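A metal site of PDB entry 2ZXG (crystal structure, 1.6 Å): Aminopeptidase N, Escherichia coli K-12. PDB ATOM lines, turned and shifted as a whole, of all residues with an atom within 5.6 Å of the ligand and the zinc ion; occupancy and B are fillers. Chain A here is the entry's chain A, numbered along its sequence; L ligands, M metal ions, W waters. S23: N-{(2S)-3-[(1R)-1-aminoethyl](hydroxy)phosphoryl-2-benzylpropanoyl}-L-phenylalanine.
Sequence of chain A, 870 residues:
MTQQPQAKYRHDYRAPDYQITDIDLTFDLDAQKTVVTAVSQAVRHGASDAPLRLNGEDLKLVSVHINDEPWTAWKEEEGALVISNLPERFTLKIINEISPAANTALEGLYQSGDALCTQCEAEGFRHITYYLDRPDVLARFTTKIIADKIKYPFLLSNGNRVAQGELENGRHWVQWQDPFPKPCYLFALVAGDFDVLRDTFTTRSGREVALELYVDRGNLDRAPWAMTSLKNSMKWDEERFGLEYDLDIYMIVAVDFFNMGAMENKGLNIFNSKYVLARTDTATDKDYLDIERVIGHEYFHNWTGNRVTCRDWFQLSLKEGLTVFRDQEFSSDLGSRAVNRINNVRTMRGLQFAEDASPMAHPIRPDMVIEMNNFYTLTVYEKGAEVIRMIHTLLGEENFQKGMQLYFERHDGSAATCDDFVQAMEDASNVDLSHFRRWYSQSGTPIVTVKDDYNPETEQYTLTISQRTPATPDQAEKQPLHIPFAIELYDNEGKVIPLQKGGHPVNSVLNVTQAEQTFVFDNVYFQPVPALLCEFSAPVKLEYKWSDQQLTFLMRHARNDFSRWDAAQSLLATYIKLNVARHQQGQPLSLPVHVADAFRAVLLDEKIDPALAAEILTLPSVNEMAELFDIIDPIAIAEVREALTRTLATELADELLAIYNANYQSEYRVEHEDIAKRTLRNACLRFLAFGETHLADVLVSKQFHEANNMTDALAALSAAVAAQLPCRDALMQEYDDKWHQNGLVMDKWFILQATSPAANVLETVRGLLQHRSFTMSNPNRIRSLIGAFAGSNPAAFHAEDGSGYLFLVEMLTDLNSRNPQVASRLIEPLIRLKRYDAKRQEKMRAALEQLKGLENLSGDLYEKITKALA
The zinc ion is bound by the side-chain carboxylate of Glu 320 (2.0 Å), an oxygen (O1) of the ligand (2.0 Å), a ring nitrogen (NE2) of His 297 (2.0 Å) and a ring nitrogen (NE2) of His 301 (2.1 Å).
A nitrogen (N1) of the ligand sits close to the side-chain amino group of Lys 319 (3.5 Å).
The side-chain hydroxyl (OH) of Tyr 381 sits close to an oxygen (O1) of the ligand (2.7 Å).
The side-chain carboxylate (OE2) of Glu 264 is in salt-bridge range of a nitrogen (N1) of the ligand.
The backbone NH (N) of Gly 261 lies within hydrogen-bond range of an oxygen (O3) of the ligand (2.9 Å).
N1 of the ligand is in salt-bridge range of OE2 of Glu 121.
The side-chain carboxylate (OE2) of Glu 298 sits close to an oxygen (O2) of the ligand (2.6 Å).
O of Ala 262 sits close to O2 of the ligand.
Asn 259 touches the ligand.
Met 260 touches the ligand.
Met 263 touches the ligand (SD to N1, 3.8 Å).
CG2 of Val 294 touches C11 of the ligand, at 3.5 Å.
Asp 327 touches the ligand.
Tyr 376 touches the ligand.
Arg 825 touches the ligand.
Hydrophobic or aromatic side chains within 4 Å of the ligand: Met 260, Met 263, Val 294, His 297, His 301, Tyr 376 and Tyr 381.
Of the 23 residues printed, 17 come within 4 Å of the ligand.
Water W3 lies within hydrogen-bond range of an oxygen (O5) of the ligand (2.7 Å) and the side-chain carboxylate of Glu 382 (3.0 Å).
Water W4 bridges the side-chain carboxylate (OE1) of Glu 382 (2.7 Å) and an oxygen (O5) of the ligand (2.9 Å).
Water W1 lies within hydrogen-bond range of O3 of the ligand (3.2 Å) and N of Gly 261 (3.2 Å).
Tyr 381 touches the zinc ion (CE2 to ZN, 3.99 Å).
Four residues have an atom within 4 Å of the zinc ion: His 297, His 301, Glu 320 and Tyr 381.
Along chain A the residues within 4 Å of the zinc ion span positions 297 to 381.
The nearest printed residue that does not touch the zinc ion is Glu 264 (4.5 Å).
The side-chain sulfur (SD) of Met 260 lies close to the side-chain amide nitrogen (NE2) of Gln 119, 3.5 Å away.
The side-chain hydroxyl of Thr 323 is in hydrogen-bond range of a ring nitrogen (ND1) of His 301.
OE1 of Glu 121 is in hydrogen-bond range of OH of Tyr 376, at 2.7 Å.
OH of Tyr 381 sits close to OE1 of Glu 320.
N of Glu 264 lies within hydrogen-bond range of OE1 of Glu 298.
O of Glu 121 lies within hydrogen-bond range of NE2 of Gln 119 (3.1 Å).
The side-chain sulfur (SD) of Met 263 is in hydrogen-bond range of the side-chain amide nitrogen (NE2) of Gln 119, at 3.6 Å.
The side-chain amino group of Lys 319 is in salt-bridge range of the side-chain carboxylate of Glu 121 (2.7 Å).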
ATOM      1  N   GLN A 119      37.202  12.030  -3.496  1.00  0.00           N
ATOM      2  CA  GLN A 119      36.808  11.552  -4.805  1.00  0.00           C
ATOM      3  C   GLN A 119      37.540  10.231  -5.040  1.00  0.00           C
ATOM      4  O   GLN A 119      38.778  10.218  -5.062  1.00  0.00           O
ATOM      5  CB  GLN A 119      37.159  12.557  -5.891  1.00  0.00           C
ATOM      6  CG  GLN A 119      36.917  12.014  -7.328  1.00  0.00           C
ATOM      7  CD  GLN A 119      35.484  11.552  -7.536  1.00  0.00           C
ATOM      8  OE1 GLN A 119      34.553  12.091  -6.930  1.00  0.00           O
ATOM      9  NE2 GLN A 119      35.290  10.560  -8.395  1.00  0.00           N
ATOM     10  N   GLU A 121      36.410   7.669  -7.567  1.00  0.00           N
ATOM     11  CA  GLU A 121      36.362   7.071  -8.921  1.00  0.00           C
ATOM     12  C   GLU A 121      37.438   7.726  -9.798  1.00  0.00           C
ATOM     13  O   GLU A 121      37.574   8.944  -9.794  1.00  0.00           O
ATOM     14  CB  GLU A 121      34.981   7.240  -9.566  1.00  0.00           C
ATOM     15  CG  GLU A 121      34.869   6.463 -10.864  1.00  0.00           C
ATOM     16  CD  GLU A 121      33.517   6.564 -11.523  1.00  0.00           C
ATOM     17  OE1 GLU A 121      33.325   5.910 -12.570  1.00  0.00           O
ATOM     18  OE2 GLU A 121      32.627   7.276 -11.016  1.00  0.00           O
ATOM     19  N   ASN A 259      37.128  17.678  -9.571  1.00  0.00           N
ATOM     20  CA  ASN A 259      37.619  17.379 -10.943  1.00  0.00           C
ATOM     21  C   ASN A 259      36.575  16.813 -11.895  1.00  0.00           C
ATOM     22  O   ASN A 259      36.895  16.383 -13.018  1.00  0.00           O
ATOM     23  CB  ASN A 259      38.759  16.357 -10.879  1.00  0.00           C
ATOM     24  CG  ASN A 259      40.068  16.943 -10.436  1.00  0.00           C
ATOM     25  OD1 ASN A 259      40.255  18.153 -10.416  1.00  0.00           O
ATOM     26  ND2 ASN A 259      40.994  16.066 -10.075  1.00  0.00           N
ATOM     27  N   MET A 260      35.333  16.732 -11.465  1.00  0.00           N
ATOM     28  CA  MET A 260      34.271  16.313 -12.386  1.00  0.00           C
ATOM     29  C   MET A 260      33.035  17.096 -12.043  1.00  0.00           C
ATOM     30  O   MET A 260      33.068  18.003 -11.197  1.00  0.00           O
ATOM     31  CB  MET A 260      34.031  14.808 -12.321  1.00  0.00           C
ATOM     32  CG  MET A 260      33.670  14.271 -10.945  1.00  0.00           C
ATOM     33  SD  MET A 260      33.558  12.452 -10.817  1.00  0.00           S
ATOM     34  CE  MET A 260      35.166  11.983 -11.441  1.00  0.00           C
ATOM     35  N   GLY A 261      31.945  16.798 -12.732  1.00  0.00           N
ATOM     36  CA  GLY A 261      30.712  17.523 -12.496  1.00  0.00           C
ATOM     37  C   GLY A 261      30.083  17.097 -11.204  1.00  0.00           C
ATOM     38  O   GLY A 261      29.576  17.936 -10.461  1.00  0.00           O
ATOM     39  N   ALA A 262      30.096  15.790 -10.940  1.00  0.00           N
ATOM     40  CA  ALA A 262      29.419  15.243  -9.761  1.00  0.00           C
ATOM     41  C   ALA A 262      29.716  13.754  -9.677  1.00  0.00           C
ATOM     42  O   ALA A 262      30.301  13.200 -10.600  1.00  0.00           O
ATOM     43  CB  ALA A 262      27.894  15.505  -9.854  1.00  0.00           C
ATOM     44  N   MET A 263      29.334  13.122  -8.565  1.00  0.00           N
ATOM     45  CA  MET A 263      29.739  11.750  -8.313  1.00  0.00           C
ATOM     46  C   MET A 263      28.694  11.019  -7.504  1.00  0.00           C
ATOM     47  O   MET A 263      28.235  11.530  -6.462  1.00  0.00           O
ATOM     48  CB  MET A 263      31.099  11.736  -7.604  1.00  0.00           C
ATOM     49  CG  MET A 263      31.579  10.342  -7.230  1.00  0.00           C
ATOM     50  SD  MET A 263      31.940   9.356  -8.730  1.00  0.00           S
ATOM     51  CE  MET A 263      31.464   7.742  -8.108  1.00  0.00           C
ATOM     52  N   GLU A 264      28.340   9.824  -7.974  1.00  0.00           N
ATOM     53  CA  GLU A 264      27.204   9.057  -7.442  1.00  0.00           C
ATOM     54  C   GLU A 264      27.481   8.241  -6.178  1.00  0.00           C
ATOM     55  O   GLU A 264      26.850   7.197  -5.995  1.00  0.00           O
ATOM     56  CB  GLU A 264      26.647   8.138  -8.536  1.00  0.00           C
ATOM     57  CG  GLU A 264      27.591   6.969  -8.953  1.00  0.00           C
ATOM     58  CD  GLU A 264      28.538   7.300 -10.108  1.00  0.00           C
ATOM     59  OE1 GLU A 264      28.993   6.334 -10.772  1.00  0.00           O
ATOM     60  OE2 GLU A 264      28.838   8.489 -10.349  1.00  0.00           O
ATOM     61  N   TYR A 275      26.957  22.447 -10.520  1.00  0.00           N
ATOM     62  CA  TYR A 275      25.787  21.650 -10.844  1.00  0.00           C
ATOM     63  C   TYR A 275      24.815  21.557  -9.671  1.00  0.00           C
ATOM     64  O   TYR A 275      23.973  20.670  -9.629  1.00  0.00           O
ATOM     65  CB  TYR A 275      26.205  20.275 -11.385  1.00  0.00           C
ATOM     66  CG  TYR A 275      26.879  20.373 -12.733  1.00  0.00           C
ATOM     67  CD1 TYR A 275      26.228  20.979 -13.812  1.00  0.00           C
ATOM     68  CD2 TYR A 275      28.163  19.890 -12.926  1.00  0.00           C
ATOM     69  CE1 TYR A 275      26.831  21.083 -15.045  1.00  0.00           C
ATOM     70  CE2 TYR A 275      28.773  19.973 -14.178  1.00  0.00           C
ATOM     71  CZ  TYR A 275      28.104  20.573 -15.226  1.00  0.00           C
ATOM     72  OH  TYR A 275      28.697  20.681 -16.467  1.00  0.00           O
ATOM     73  N   ARG A 293      19.778  18.134 -15.163  1.00  0.00           N
ATOM     74  CA  ARG A 293      20.260  16.927 -15.800  1.00  0.00           C
ATOM     75  C   ARG A 293      21.343  16.231 -14.985  1.00  0.00           C
ATOM     76  O   ARG A 293      21.391  15.011 -15.004  1.00  0.00           O
ATOM     77  CB  ARG A 293      20.703  17.214 -17.246  1.00  0.00           C
ATOM     78  CG  ARG A 293      22.150  17.527 -17.423  1.00  0.00           C
ATOM     79  CD  ARG A 293      22.462  17.790 -18.911  1.00  0.00           C
ATOM     80  NE  ARG A 293      22.031  19.134 -19.312  1.00  0.00           N
ATOM     81  CZ  ARG A 293      20.963  19.407 -20.065  1.00  0.00           C
ATOM     82  NH1 ARG A 293      20.182  18.442 -20.536  1.00  0.00           N
ATOM     83  NH2 ARG A 293      20.680  20.678 -20.358  1.00  0.00           N
ATOM     84  N   VAL A 294      22.193  16.978 -14.277  1.00  0.00           N
ATOM     85  CA  VAL A 294      23.276  16.355 -13.495  1.00  0.00           C
ATOM     86  C   VAL A 294      22.736  15.791 -12.186  1.00  0.00           C
ATOM     87  O   VAL A 294      23.106  14.679 -11.784  1.00  0.00           O
ATOM     88  CB  VAL A 294      24.472  17.313 -13.284  1.00  0.00           C
ATOM     89  CG1 VAL A 294      25.549  16.662 -12.413  1.00  0.00           C
ATOM     90  CG2 VAL A 294      25.081  17.684 -14.641  1.00  0.00           C
ATOM     91  N   HIS A 297      21.232  12.688 -13.432  1.00  0.00           N
ATOM     92  CA  HIS A 297      22.285  11.726 -13.752  1.00  0.00           C
ATOM     93  C   HIS A 297      22.782  10.984 -12.495  1.00  0.00           C
ATOM     94  O   HIS A 297      22.838   9.754 -12.470  1.00  0.00           O
ATOM     95  CB  HIS A 297      23.447  12.474 -14.411  1.00  0.00           C
ATOM     96  CG  HIS A 297      24.547  11.603 -14.920  1.00  0.00           C
ATOM     97  ND1 HIS A 297      24.636  11.217 -16.244  1.00  0.00           N
ATOM     98  CD2 HIS A 297      25.618  11.066 -14.303  1.00  0.00           C
ATOM     99  CE1 HIS A 297      25.712  10.460 -16.409  1.00  0.00           C
ATOM    100  NE2 HIS A 297      26.332  10.360 -15.243  1.00  0.00           N
ATOM    101  N   GLU A 298      23.144  11.747 -11.457  1.00  0.00           N
ATOM    102  CA  GLU A 298      23.681  11.132 -10.253  1.00  0.00           C
ATOM    103  C   GLU A 298      22.634  10.258  -9.591  1.00  0.00           C
ATOM    104  O   GLU A 298      22.948   9.143  -9.133  1.00  0.00           O
ATOM    105  CB  GLU A 298      24.217  12.179  -9.277  1.00  0.00           C
ATOM    106  CG  GLU A 298      25.326  13.040  -9.893  1.00  0.00           C
ATOM    107  CD  GLU A 298      26.447  12.240 -10.519  1.00  0.00           C
ATOM    108  OE1 GLU A 298      26.748  11.112 -10.053  1.00  0.00           O
ATOM    109  OE2 GLU A 298      27.015  12.748 -11.500  1.00  0.00           O
ATOM    110  N   HIS A 301      22.263   6.965 -11.457  1.00  0.00           N
ATOM    111  CA  HIS A 301      23.356   6.033 -11.167  1.00  0.00           C
ATOM    112  C   HIS A 301      23.031   5.115  -9.983  1.00  0.00           C
ATOM    113  O   HIS A 301      23.654   4.060  -9.841  1.00  0.00           O
ATOM    114  CB  HIS A 301      24.645   6.777 -10.840  1.00  0.00           C
ATOM    115  CG  HIS A 301      25.544   7.050 -12.015  1.00  0.00           C
ATOM    116  ND1 HIS A 301      25.919   6.081 -12.913  1.00  0.00           N
ATOM    117  CD2 HIS A 301      26.234   8.164 -12.353  1.00  0.00           C
ATOM    118  CE1 HIS A 301      26.759   6.607 -13.795  1.00  0.00           C
ATOM    119  NE2 HIS A 301      26.974   7.859 -13.464  1.00  0.00           N
ATOM    120  N   LYS A 319      27.705   1.668 -17.196  1.00  0.00           N
ATOM    121  CA  LYS A 319      27.008   2.636 -16.350  1.00  0.00           C
ATOM    122  C   LYS A 319      26.909   4.015 -16.979  1.00  0.00           C
ATOM    123  O   LYS A 319      25.887   4.684 -16.798  1.00  0.00           O
ATOM    124  CB  LYS A 319      27.590   2.686 -14.923  1.00  0.00           C
ATOM    125  CG  LYS A 319      28.969   3.307 -14.741  1.00  0.00           C
ATOM    126  CD  LYS A 319      29.328   3.245 -13.227  1.00  0.00           C
ATOM    127  CE  LYS A 319      30.693   3.826 -12.895  1.00  0.00           C
ATOM    128  NZ  LYS A 319      30.741   5.335 -12.885  1.00  0.00           N
ATOM    129  N   GLU A 320      27.934   4.456 -17.719  1.00  0.00           N
ATOM    130  CA  GLU A 320      27.908   5.852 -18.193  1.00  0.00           C
ATOM    131  C   GLU A 320      27.059   6.044 -19.441  1.00  0.00           C
ATOM    132  O   GLU A 320      26.288   7.018 -19.502  1.00  0.00           O
ATOM    133  CB  GLU A 320      29.309   6.414 -18.391  1.00  0.00           C
ATOM    134  CG  GLU A 320      30.136   6.464 -17.115  1.00  0.00           C
ATOM    135  CD  GLU A 320      29.481   7.253 -15.989  1.00  0.00           C
ATOM    136  OE1 GLU A 320      29.906   7.091 -14.828  1.00  0.00           O
ATOM    137  OE2 GLU A 320      28.551   8.062 -16.251  1.00  0.00           O
ATOM    138  N   THR A 323      23.483   5.650 -18.111  1.00  0.00           N
ATOM    139  CA  THR A 323      23.059   6.754 -17.243  1.00  0.00           C
ATOM    140  C   THR A 323      22.918   8.051 -18.033  1.00  0.00           C
ATOM    141  O   THR A 323      22.015   8.838 -17.732  1.00  0.00           O
ATOM    142  CB  THR A 323      23.975   6.892 -16.006  1.00  0.00           C
ATOM    143  OG1 THR A 323      23.959   5.632 -15.299  1.00  0.00           O
ATOM    144  CG2 THR A 323      23.489   8.001 -15.083  1.00  0.00           C
ATOM    145  N   ASP A 327      19.654  10.297 -18.294  1.00  0.00           N
ATOM    146  CA  ASP A 327      19.552  11.738 -18.050  1.00  0.00           C
ATOM    147  C   ASP A 327      18.969  12.464 -19.269  1.00  0.00           C
ATOM    148  O   ASP A 327      18.232  13.424 -19.116  1.00  0.00           O
ATOM    149  CB  ASP A 327      20.833  12.381 -17.447  1.00  0.00           C
ATOM    150  CG  ASP A 327      21.922  12.743 -18.488  1.00  0.00           C
ATOM    151  OD1 ASP A 327      23.111  12.408 -18.231  1.00  0.00           O
ATOM    152  OD2 ASP A 327      21.628  13.450 -19.480  1.00  0.00           O
ATOM    153  N   TYR A 376      37.117   8.837 -19.392  1.00  0.00           N
ATOM    154  CA  TYR A 376      35.815   9.432 -19.058  1.00  0.00           C
ATOM    155  C   TYR A 376      35.457  10.381 -20.196  1.00  0.00           C
ATOM    156  O   TYR A 376      35.470  11.594 -20.054  1.00  0.00           O
ATOM    157  CB  TYR A 376      35.884  10.103 -17.657  1.00  0.00           C
ATOM    158  CG  TYR A 376      35.848   9.016 -16.604  1.00  0.00           C
ATOM    159  CD1 TYR A 376      36.982   8.211 -16.366  1.00  0.00           C
ATOM    160  CD2 TYR A 376      34.669   8.723 -15.914  1.00  0.00           C
ATOM    161  CE1 TYR A 376      36.940   7.171 -15.436  1.00  0.00           C
ATOM    162  CE2 TYR A 376      34.624   7.693 -14.974  1.00  0.00           C
ATOM    163  CZ  TYR A 376      35.762   6.935 -14.752  1.00  0.00           C
ATOM    164  OH  TYR A 376      35.726   5.890 -13.867  1.00  0.00           O
ATOM    165  N   TYR A 381      30.698   8.179 -22.816  1.00  0.00           N
ATOM    166  CA  TYR A 381      29.466   8.829 -22.346  1.00  0.00           C
ATOM    167  C   TYR A 381      28.444   9.022 -23.450  1.00  0.00           C
ATOM    168  O   TYR A 381      27.384   8.375 -23.460  1.00  0.00           O
ATOM    169  CB  TYR A 381      29.808  10.192 -21.709  1.00  0.00           C
ATOM    170  CG  TYR A 381      30.283  10.083 -20.283  1.00  0.00           C
ATOM    171  CD1 TYR A 381      31.506   9.498 -19.978  1.00  0.00           C
ATOM    172  CD2 TYR A 381      29.497  10.585 -19.244  1.00  0.00           C
ATOM    173  CE1 TYR A 381      31.925   9.383 -18.640  1.00  0.00           C
ATOM    174  CE2 TYR A 381      29.907  10.493 -17.932  1.00  0.00           C
ATOM    175  CZ  TYR A 381      31.131   9.882 -17.641  1.00  0.00           C
ATOM    176  OH  TYR A 381      31.538   9.773 -16.334  1.00  0.00           O
ATOM    177  N   GLU A 382      28.764   9.915 -24.402  1.00  0.00           N
ATOM    178  CA  GLU A 382      27.783  10.321 -25.405  1.00  0.00           C
ATOM    179  C   GLU A 382      27.594   9.285 -26.509  1.00  0.00           C
ATOM    180  O   GLU A 382      26.441   8.967 -26.857  1.00  0.00           O
ATOM    181  CB  GLU A 382      28.126  11.692 -25.982  1.00  0.00           C
ATOM    182  CG  GLU A 382      27.591  12.860 -25.157  1.00  0.00           C
ATOM    183  CD  GLU A 382      28.489  13.309 -24.015  1.00  0.00           C
ATOM    184  OE1 GLU A 382      29.610  12.762 -23.848  1.00  0.00           O
ATOM    185  OE2 GLU A 382      28.070  14.250 -23.291  1.00  0.00           O
ATOM    186  N   GLN A 821      44.710  15.238 -13.784  1.00  0.00           N
ATOM    187  CA  GLN A 821      43.411  15.014 -14.436  1.00  0.00           C
ATOM    188  C   GLN A 821      42.969  16.254 -15.192  1.00  0.00           C
ATOM    189  O   GLN A 821      42.521  16.170 -16.338  1.00  0.00           O
ATOM    190  CB  GLN A 821      42.335  14.638 -13.418  1.00  0.00           C
ATOM    191  CG  GLN A 821      42.218  13.184 -13.216  1.00  0.00           C
ATOM    192  CD  GLN A 821      41.098  12.868 -12.242  1.00  0.00           C
ATOM    193  OE1 GLN A 821      39.970  12.551 -12.645  1.00  0.00           O
ATOM    194  NE2 GLN A 821      41.402  12.983 -10.960  1.00  0.00           N
ATOM    195  N   ARG A 825      42.620  16.906 -19.415  1.00  0.00           N
ATOM    196  CA  ARG A 825      41.474  17.503 -20.121  1.00  0.00           C
ATOM    197  C   ARG A 825      41.967  18.641 -21.011  1.00  0.00           C
ATOM    198  O   ARG A 825      41.516  18.791 -22.158  1.00  0.00           O
ATOM    199  CB  ARG A 825      40.428  18.037 -19.135  1.00  0.00           C
ATOM    200  CG  ARG A 825      39.647  16.958 -18.439  1.00  0.00           C
ATOM    201  CD  ARG A 825      38.427  17.556 -17.726  1.00  0.00           C
ATOM    202  NE  ARG A 825      37.261  17.662 -18.615  1.00  0.00           N
ATOM    203  CZ  ARG A 825      36.081  18.176 -18.248  1.00  0.00           C
ATOM    204  NH1 ARG A 825      35.899  18.647 -17.025  1.00  0.00           N
ATOM    205  NH2 ARG A 825      35.088  18.211 -19.129  1.00  0.00           N
HETATM  206  O2  S23 L   1      28.647  11.034 -12.605  1.00  0.00           O
HETATM  207  P   S23 L   1      29.878  11.005 -13.332  1.00  0.00           P
HETATM  208  O1  S23 L   1      29.588  10.243 -14.543  1.00  0.00           O
HETATM  209  C1  S23 L   1      30.964  10.183 -12.471  1.00  0.00           C
HETATM  210  N1  S23 L   1      30.664   8.764 -12.297  1.00  0.00           N
HETATM  211  C2  S23 L   1      32.389  10.174 -13.046  1.00  0.00           C
HETATM  212  C3  S23 L   1      30.428  12.459 -13.691  1.00  0.00           C
HETATM  213  C4  S23 L   1      29.711  13.282 -14.797  1.00  0.00           C
HETATM  214  C6  S23 L   1      28.527  14.125 -14.247  1.00  0.00           C
HETATM  215  C7  S23 L   1      27.807  14.837 -15.386  1.00  0.00           C
HETATM  216  C8  S23 L   1      26.748  14.189 -16.042  1.00  0.00           C
HETATM  217  C10 S23 L   1      26.081  14.819 -17.088  1.00  0.00           C
HETATM  218  C12 S23 L   1      26.490  16.085 -17.494  1.00  0.00           C
HETATM  219  C11 S23 L   1      27.548  16.747 -16.864  1.00  0.00           C
HETATM  220  C9  S23 L   1      28.208  16.123 -15.795  1.00  0.00           C
HETATM  221  C5  S23 L   1      30.632  14.213 -15.583  1.00  0.00           C
HETATM  222  O3  S23 L   1      31.278  15.097 -15.036  1.00  0.00           O
HETATM  223  N2  S23 L   1      30.664  14.022 -16.907  1.00  0.00           N
HETATM  224  C13 S23 L   1      31.290  14.958 -17.835  1.00  0.00           C
HETATM  225  C14 S23 L   1      30.373  15.230 -18.992  1.00  0.00           C
HETATM  226  O4  S23 L   1      30.433  16.352 -19.542  1.00  0.00           O
HETATM  227  O5  S23 L   1      29.586  14.334 -19.369  1.00  0.00           O
HETATM  228  C15 S23 L   1      32.617  14.405 -18.370  1.00  0.00           C
HETATM  229  C16 S23 L   1      33.637  14.169 -17.286  1.00  0.00           C
HETATM  230  C17 S23 L   1      34.486  15.207 -16.885  1.00  0.00           C
HETATM  231  C19 S23 L   1      35.445  14.990 -15.884  1.00  0.00           C
HETATM  232  C21 S23 L   1      35.550  13.729 -15.279  1.00  0.00           C
HETATM  233  C20 S23 L   1      34.678  12.695 -15.662  1.00  0.00           C
HETATM  234  C18 S23 L   1      33.728  12.909 -16.677  1.00  0.00           C
HETATM  235 ZN    ZN M   1      27.902   9.160 -14.749  1.00  0.00          ZN
HETATM  236  O   HOH W   1      31.916  18.146 -15.615  1.00  0.00           O
HETATM  237  O   HOH W   2      33.910  13.595 -21.485  1.00  0.00           O
HETATM  238  O   HOH W   3      27.204  13.824 -20.450  1.00  0.00           O
HETATM  239  O   HOH W   4      31.045  13.549 -21.722  1.00  0.00           O
